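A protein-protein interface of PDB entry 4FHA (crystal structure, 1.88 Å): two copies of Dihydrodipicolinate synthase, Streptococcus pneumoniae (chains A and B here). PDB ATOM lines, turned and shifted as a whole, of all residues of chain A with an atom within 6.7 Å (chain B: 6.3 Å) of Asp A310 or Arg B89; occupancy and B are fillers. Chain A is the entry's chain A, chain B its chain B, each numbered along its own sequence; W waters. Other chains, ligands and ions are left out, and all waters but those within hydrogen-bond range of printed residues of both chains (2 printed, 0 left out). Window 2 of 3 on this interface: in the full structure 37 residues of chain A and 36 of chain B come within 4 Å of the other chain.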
ATOM      1  N   ASP A  22       2.367  41.712 -26.199  1.00  0.00           N
ATOM      2  CA  ASP A  22       2.394  40.702 -25.131  1.00  0.00           C
ATOM      3  C   ASP A  22       1.612  39.427 -25.470  1.00  0.00           C
ATOM      4  O   ASP A  22       1.694  38.431 -24.746  1.00  0.00           O
ATOM      5  CB  ASP A  22       1.936  41.292 -23.783  1.00  0.00           C
ATOM      6  CG  ASP A  22       0.483  41.775 -23.788  1.00  0.00           C
ATOM      7  OD1 ASP A  22      -0.310  41.398 -24.678  1.00  0.00           O
ATOM      8  OD2 ASP A  22       0.128  42.541 -22.870  1.00  0.00           O
ATOM      9  N   THR A  56      -5.180  29.784 -33.128  1.00  0.00           N
ATOM     10  CA  THR A  56      -4.451  30.224 -31.932  1.00  0.00           C
ATOM     11  C   THR A  56      -5.333  31.037 -30.986  1.00  0.00           C
ATOM     12  O   THR A  56      -4.870  31.522 -29.954  1.00  0.00           O
ATOM     13  CB  THR A  56      -3.172  31.020 -32.281  1.00  0.00           C
ATOM     14  OG1 THR A  56      -3.520  32.207 -33.002  1.00  0.00           O
ATOM     15  CG2 THR A  56      -2.213  30.172 -33.107  1.00  0.00           C
ATOM     16  N   LEU A 274       2.357  32.556 -32.199  1.00  0.00           N
ATOM     17  CA  LEU A 274       3.026  31.302 -32.528  1.00  0.00           C
ATOM     18  C   LEU A 274       1.991  30.189 -32.724  1.00  0.00           C
ATOM     19  O   LEU A 274       0.989  30.147 -32.004  1.00  0.00           O
ATOM     20  CB  LEU A 274       4.045  30.930 -31.450  1.00  0.00           C
ATOM     21  CG  LEU A 274       5.404  31.630 -31.481  1.00  0.00           C
ATOM     22  CD1 LEU A 274       6.255  31.198 -30.294  1.00  0.00           C
ATOM     23  CD2 LEU A 274       6.135  31.354 -32.789  1.00  0.00           C
ATOM     24  N   PRO A 275       2.231  29.266 -33.673  1.00  0.00           N
ATOM     25  CA  PRO A 275       3.447  28.974 -34.439  1.00  0.00           C
ATOM     26  C   PRO A 275       3.758  29.900 -35.621  1.00  0.00           C
ATOM     27  O   PRO A 275       4.751  29.681 -36.312  1.00  0.00           O
ATOM     28  CB  PRO A 275       3.195  27.556 -34.944  1.00  0.00           C
ATOM     29  CG  PRO A 275       1.719  27.498 -35.127  1.00  0.00           C
ATOM     30  CD  PRO A 275       1.120  28.377 -34.064  1.00  0.00           C
ATOM     31  N   VAL A 306       4.398  35.598 -30.944  1.00  0.00           N
ATOM     32  CA  VAL A 306       3.986  35.874 -29.569  1.00  0.00           C
ATOM     33  C   VAL A 306       2.977  34.832 -29.063  1.00  0.00           C
ATOM     34  O   VAL A 306       2.439  34.052 -29.846  1.00  0.00           O
ATOM     35  CB  VAL A 306       3.459  37.320 -29.420  1.00  0.00           C
ATOM     36  CG1 VAL A 306       3.413  37.725 -27.963  1.00  0.00           C
ATOM     37  CG2 VAL A 306       4.367  38.295 -30.161  1.00  0.00           C
ATOM     38  N   LEU A 307       2.747  34.811 -27.751  1.00  0.00           N
ATOM     39  CA  LEU A 307       1.886  33.810 -27.123  1.00  0.00           C
ATOM     40  C   LEU A 307       0.722  34.437 -26.367  1.00  0.00           C
ATOM     41  O   LEU A 307       0.865  35.505 -25.770  1.00  0.00           O
ATOM     42  CB  LEU A 307       2.702  32.945 -26.156  1.00  0.00           C
ATOM     43  CG  LEU A 307       3.820  32.073 -26.726  1.00  0.00           C
ATOM     44  CD1 LEU A 307       4.883  31.800 -25.671  1.00  0.00           C
ATOM     45  CD2 LEU A 307       3.250  30.774 -27.277  1.00  0.00           C
ATOM     46  N   ARG A 308      -0.425  33.759 -26.394  1.00  0.00           N
ATOM     47  CA  ARG A 308      -1.569  34.115 -25.562  1.00  0.00           C
ATOM     48  C   ARG A 308      -1.113  34.079 -24.100  1.00  0.00           C
ATOM     49  O   ARG A 308      -0.448  33.127 -23.693  1.00  0.00           O
ATOM     50  CB  ARG A 308      -2.724  33.128 -25.785  1.00  0.00           C
ATOM     51  CG  ARG A 308      -4.046  33.541 -25.153  1.00  0.00           C
ATOM     52  CD  ARG A 308      -5.153  32.536 -25.441  1.00  0.00           C
ATOM     53  NE  ARG A 308      -5.196  31.449 -24.465  1.00  0.00           N
ATOM     54  CZ  ARG A 308      -4.814  30.196 -24.702  1.00  0.00           C
ATOM     55  NH1 ARG A 308      -4.361  29.843 -25.897  1.00  0.00           N
ATOM     56  NH2 ARG A 308      -4.896  29.287 -23.740  1.00  0.00           N
ATOM     57  N   PRO A 309      -1.435  35.130 -23.323  1.00  0.00           N
ATOM     58  CA  PRO A 309      -1.023  35.200 -21.917  1.00  0.00           C
ATOM     59  C   PRO A 309      -1.509  34.013 -21.081  1.00  0.00           C
ATOM     60  O   PRO A 309      -2.692  33.667 -21.128  1.00  0.00           O
ATOM     61  CB  PRO A 309      -1.677  36.495 -21.429  1.00  0.00           C
ATOM     62  CG  PRO A 309      -1.772  37.342 -22.651  1.00  0.00           C
ATOM     63  CD  PRO A 309      -2.096  36.376 -23.757  1.00  0.00           C
ATOM     64  N   ASP A 310      -0.593  33.399 -20.331  1.00  0.00           N
ATOM     65  CA  ASP A 310      -0.942  32.316 -19.405  1.00  0.00           C
ATOM     66  C   ASP A 310      -1.352  32.862 -18.029  1.00  0.00           C
ATOM     67  O   ASP A 310      -1.126  32.229 -16.991  1.00  0.00           O
ATOM     68  CB  ASP A 310       0.197  31.287 -19.298  1.00  0.00           C
ATOM     69  CG  ASP A 310       1.499  31.885 -18.770  1.00  0.00           C
ATOM     70  OD1 ASP A 310       2.173  31.202 -17.966  1.00  0.00           O
ATOM     71  OD2 ASP A 310       1.856  33.021 -19.156  1.00  0.00           O
ATOM     72  N   TYR A 311      -1.973  34.038 -18.043  1.00  0.00           N
ATOM     73  CA  TYR A 311      -2.434  34.710 -16.835  1.00  0.00           C
ATOM     74  C   TYR A 311      -3.719  35.487 -17.117  1.00  0.00           C
ATOM     75  O   TYR A 311      -4.111  35.675 -18.271  1.00  0.00           O
ATOM     76  CB  TYR A 311      -1.344  35.638 -16.283  1.00  0.00           C
ATOM     77  CG  TYR A 311      -0.862  36.694 -17.259  1.00  0.00           C
ATOM     78  CD1 TYR A 311      -1.540  37.909 -17.396  1.00  0.00           C
ATOM     79  CD2 TYR A 311       0.273  36.482 -18.042  1.00  0.00           C
ATOM     80  CE1 TYR A 311      -1.103  38.878 -18.285  1.00  0.00           C
ATOM     81  CE2 TYR A 311       0.720  37.449 -18.932  1.00  0.00           C
ATOM     82  CZ  TYR A 311       0.027  38.644 -19.050  1.00  0.00           C
ATOM     83  OH  TYR A 311       0.461  39.605 -19.932  1.00  0.00           O
ATOM     84  OXT TYR A 311      -4.401  35.949 -16.203  1.00  0.00           O
ATOM     85  N   ASP B  87      -1.382  25.147 -31.806  1.00  0.00           N
ATOM     86  CA  ASP B  87      -1.442  26.316 -30.941  1.00  0.00           C
ATOM     87  C   ASP B  87      -0.296  26.175 -29.941  1.00  0.00           C
ATOM     88  O   ASP B  87      -0.326  25.303 -29.068  1.00  0.00           O
ATOM     89  CB  ASP B  87      -2.811  26.356 -30.238  1.00  0.00           C
ATOM     90  CG  ASP B  87      -2.992  27.565 -29.318  1.00  0.00           C
ATOM     91  OD1 ASP B  87      -2.000  28.167 -28.860  1.00  0.00           O
ATOM     92  OD2 ASP B  87      -4.159  27.901 -29.031  1.00  0.00           O
ATOM     93  N   THR B  88       0.727  27.014 -30.094  1.00  0.00           N
ATOM     94  CA  THR B  88       1.923  26.931 -29.253  1.00  0.00           C
ATOM     95  C   THR B  88       1.604  27.087 -27.758  1.00  0.00           C
ATOM     96  O   THR B  88       2.067  26.284 -26.948  1.00  0.00           O
ATOM     97  CB  THR B  88       3.011  27.923 -29.704  1.00  0.00           C
ATOM     98  OG1 THR B  88       3.161  27.843 -31.126  1.00  0.00           O
ATOM     99  CG2 THR B  88       4.353  27.606 -29.044  1.00  0.00           C
ATOM    100  N   ARG B  89       0.803  28.093 -27.405  1.00  0.00           N
ATOM    101  CA  ARG B  89       0.386  28.292 -26.010  1.00  0.00           C
ATOM    102  C   ARG B  89      -0.320  27.054 -25.440  1.00  0.00           C
ATOM    103  O   ARG B  89       0.033  26.586 -24.355  1.00  0.00           O
ATOM    104  CB  ARG B  89      -0.476  29.558 -25.850  1.00  0.00           C
ATOM    105  CG  ARG B  89      -1.174  29.713 -24.497  1.00  0.00           C
ATOM    106  CD  ARG B  89      -0.208  29.697 -23.316  1.00  0.00           C
ATOM    107  NE  ARG B  89       0.584  30.921 -23.219  1.00  0.00           N
ATOM    108  CZ  ARG B  89       1.731  31.029 -22.556  1.00  0.00           C
ATOM    109  NH1 ARG B  89       2.248  29.980 -21.926  1.00  0.00           N
ATOM    110  NH2 ARG B  89       2.371  32.191 -22.530  1.00  0.00           N
ATOM    111  N   ASP B  90      -1.299  26.525 -26.178  1.00  0.00           N
ATOM    112  CA  ASP B  90      -1.990  25.291 -25.785  1.00  0.00           C
ATOM    113  C   ASP B  90      -1.010  24.136 -25.558  1.00  0.00           C
ATOM    114  O   ASP B  90      -1.113  23.410 -24.561  1.00  0.00           O
ATOM    115  CB  ASP B  90      -3.040  24.903 -26.831  1.00  0.00           C
ATOM    116  CG  ASP B  90      -3.742  23.596 -26.501  1.00  0.00           C
ATOM    117  OD1 ASP B  90      -4.577  23.580 -25.572  1.00  0.00           O
ATOM    118  OD2 ASP B  90      -3.460  22.584 -27.178  1.00  0.00           O
ATOM    119  N   SER B  91      -0.061  23.982 -26.479  1.00  0.00           N
ATOM    120  CA  SER B  91       0.951  22.929 -26.401  1.00  0.00           C
ATOM    121  C   SER B  91       1.850  23.109 -25.178  1.00  0.00           C
ATOM    122  O   SER B  91       2.207  22.132 -24.515  1.00  0.00           O
ATOM    123  CB  SER B  91       1.797  22.898 -27.676  1.00  0.00           C
ATOM    124  OG  SER B  91       0.998  22.674 -28.827  1.00  0.00           O
ATOM    125  N   ILE B  92       2.208  24.359 -24.891  1.00  0.00           N
ATOM    126  CA  ILE B  92       3.023  24.697 -23.721  1.00  0.00           C
ATOM    127  C   ILE B  92       2.308  24.322 -22.423  1.00  0.00           C
ATOM    128  O   ILE B  92       2.898  23.684 -21.549  1.00  0.00           O
ATOM    129  CB  ILE B  92       3.405  26.197 -23.704  1.00  0.00           C
ATOM    130  CG1 ILE B  92       4.481  26.488 -24.754  1.00  0.00           C
ATOM    131  CG2 ILE B  92       3.898  26.627 -22.324  1.00  0.00           C
ATOM    132  CD1 ILE B  92       4.682  27.962 -25.028  1.00  0.00           C
ATOM    133  N   GLU B  93       1.040  24.711 -22.310  1.00  0.00           N
ATOM    134  CA  GLU B  93       0.265  24.453 -21.097  1.00  0.00           C
ATOM    135  C   GLU B  93       0.019  22.961 -20.886  1.00  0.00           C
ATOM    136  O   GLU B  93       0.096  22.472 -19.756  1.00  0.00           O
ATOM    137  CB  GLU B  93      -1.058  25.228 -21.102  1.00  0.00           C
ATOM    138  CG  GLU B  93      -0.920  26.750 -21.124  1.00  0.00           C
ATOM    139  CD  GLU B  93      -0.029  27.303 -20.017  1.00  0.00           C
ATOM    140  OE1 GLU B  93      -0.379  27.159 -18.824  1.00  0.00           O
ATOM    141  OE2 GLU B  93       1.021  27.896 -20.343  1.00  0.00           O
ATOM    142  N   PHE B  94      -0.253  22.237 -21.969  1.00  0.00           N
ATOM    143  CA  PHE B  94      -0.519  20.805 -21.861  1.00  0.00           C
ATOM    144  C   PHE B  94       0.718  19.961 -21.539  1.00  0.00           C
ATOM    145  O   PHE B  94       0.624  19.009 -20.765  1.00  0.00           O
ATOM    146  CB  PHE B  94      -1.248  20.256 -23.093  1.00  0.00           C
ATOM    147  CG  PHE B  94      -1.763  18.854 -22.907  1.00  0.00           C
ATOM    148  CD1 PHE B  94      -2.709  18.569 -21.920  1.00  0.00           C
ATOM    149  CD2 PHE B  94      -1.302  17.818 -23.709  1.00  0.00           C
ATOM    150  CE1 PHE B  94      -3.182  17.275 -21.744  1.00  0.00           C
ATOM    151  CE2 PHE B  94      -1.773  16.524 -23.538  1.00  0.00           C
ATOM    152  CZ  PHE B  94      -2.716  16.252 -22.555  1.00  0.00           C
ATOM    153  N   LYS B  96       3.243  20.960 -19.850  1.00  0.00           N
ATOM    154  CA  LYS B  96       3.461  21.250 -18.436  1.00  0.00           C
ATOM    155  C   LYS B  96       2.599  20.344 -17.561  1.00  0.00           C
ATOM    156  O   LYS B  96       3.086  19.784 -16.579  1.00  0.00           O
ATOM    157  CB  LYS B  96       3.177  22.721 -18.127  1.00  0.00           C
ATOM    158  CG  LYS B  96       4.327  23.657 -18.458  1.00  0.00           C
ATOM    159  CD  LYS B  96       4.011  25.079 -18.028  1.00  0.00           C
ATOM    160  CE  LYS B  96       5.204  25.994 -18.239  1.00  0.00           C
ATOM    161  NZ  LYS B  96       4.885  27.402 -17.881  1.00  0.00           N
ATOM    162  N   HIS B 125       8.052  27.498 -32.365  1.00  0.00           N
ATOM    163  CA  HIS B 125       6.993  26.643 -31.817  1.00  0.00           C
ATOM    164  C   HIS B 125       7.562  25.504 -31.009  1.00  0.00           C
ATOM    165  O   HIS B 125       7.170  25.301 -29.853  1.00  0.00           O
ATOM    166  CB  HIS B 125       6.096  26.123 -32.944  1.00  0.00           C
ATOM    167  CG  HIS B 125       5.116  25.053 -32.515  1.00  0.00           C
ATOM    168  ND1 HIS B 125       3.929  25.340 -31.955  1.00  0.00           N
ATOM    169  CD2 HIS B 125       5.178  23.662 -32.613  1.00  0.00           C
ATOM    170  CE1 HIS B 125       3.269  24.196 -31.691  1.00  0.00           C
ATOM    171  NE2 HIS B 125       4.032  23.171 -32.100  1.00  0.00           N
HETATM  172  O   HOH W   1      -3.176  30.557 -28.063  1.00  0.00           O
HETATM  173  O   HOH W   2       0.526  30.117 -29.280  1.00  0.00           O
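The side-chain hydroxyl (OG) of Ser B91 lies within hydrogen-bond range of the backbone carbonyl oxygen (O) of Asp B87, 3.0 Å away. The backbone NH of Leu A274 is in hydrogen-bond range of the backbone carbonyl oxygen of Val A306, at 2.8 Å. The backbone NH (N) of Asp B90 lies within hydrogen-bond range of the side-chain carboxylate (OD1) of Asp B87 (3.2 Å). The side-chain hydroxyl (OG1) of Thr B88 is in hydrogen-bond range of a ring nitrogen (ND1) of His B125. The guanidinium group (NH1) of Arg B89 lies within salt-bridge range of the side-chain carboxylate (OE2) of Glu B93, 2.9 Å away. The side-chain carboxylate of Asp B87 lies within hydrogen-bond range of the backbone NH of Arg B89, 3.2 Å away.
Asp A310 touches just these residues of chain B: Arg B89 and Glu B93. Arg B89 touches just these residues of chain A: Leu A307, Arg A308 and Asp A310. Printed residues of chain B within 4 Å of Thr A56: Asp B87. Of the printed residues of chain A, Asp B87 touches Thr A56 (3.7 Å) and Arg A308 (3.7 Å). Printed residues of chain A within 4 Å of Ile B92: Leu A307. Of the printed residues of chain B, Leu A307 touches Thr B88 (3.8 Å), Arg B89 (3.6 Å) and Ile B92 (3.9 Å). Asp A22 touches none of the printed residues of chain B. The nearest residue of chain A that does not touch Arg B89 is Pro A309 (4.3 Å).
Asp B87 touches Thr A56. CB of Pro A275 touches ND1 of His B125, at 3.8 Å. Leu A307 touches Thr B88 (CD2 to CB, 3.8 Å). Arg B89 touches Leu A307. CD1 of Ile B92 touches CD2 of Leu A307 (3.9 Å). OE2 of Glu B93 touches CB of Asp A310, at 3.6 Å.
The side-chain hydroxyl (OG1) of Thr B88 lies close to the backbone carbonyl oxygen (O) of Leu A274 (3.3 Å). The guanidinium group of Arg B89 is in hydrogen-bond range of the backbone carbonyl oxygen of Arg A308 (2.5 Å). The side-chain carboxylate (OD2) of Asp B87 lies within salt-bridge range of the guanidinium group (NH1) of Arg A308 (3.7 Å). The side-chain hydroxyl (OG1) of Thr B88 sits close to the backbone nitrogen (N) of Pro A275, 3.1 Å away. The side-chain carboxylate (OD2) of Asp A310 lies within salt-bridge range of the guanidinium group (NH2) of Arg B89.
Water W1 lies within hydrogen-bond range of the guanidinium group of Arg A308 (2.6 Å), the backbone carbonyl oxygen of Thr A56 (2.7 Å) and the side-chain carboxylate of Asp B87 (2.8 Å). Water W2 lies within hydrogen-bond range of O of Leu A274 (2.8 Å), N of Arg B89 (2.8 Å), N of Thr B88 (3.2 Å) and OD1 of Asp B87 (3.2 Å).
Of the 10 printed residues of chain B, 6 touch a printed residue of chain A. Hydrophobic or aromatic side chains of chain B within 4 Å of the printed part of chain A: Ile B92 and His B125. Of the 10 printed residues of chain A, 6 touch a printed residue of chain B. Hydrophobic or aromatic side chains of chain A that line the printed part of chain B: Leu A274, Pro A275 and Leu A307. Among the printed residues, Asp or Glu carboxylates within 4 Å of a Lys or Arg side-chain nitrogen of the other chain: Arg A308 with Asp B87 and Asp A310 with Arg B89.
No position is printed for both chains. Of the 11 pairs that touch across the chains among the printed residues, none has its exchanged pair printed and touching as well.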
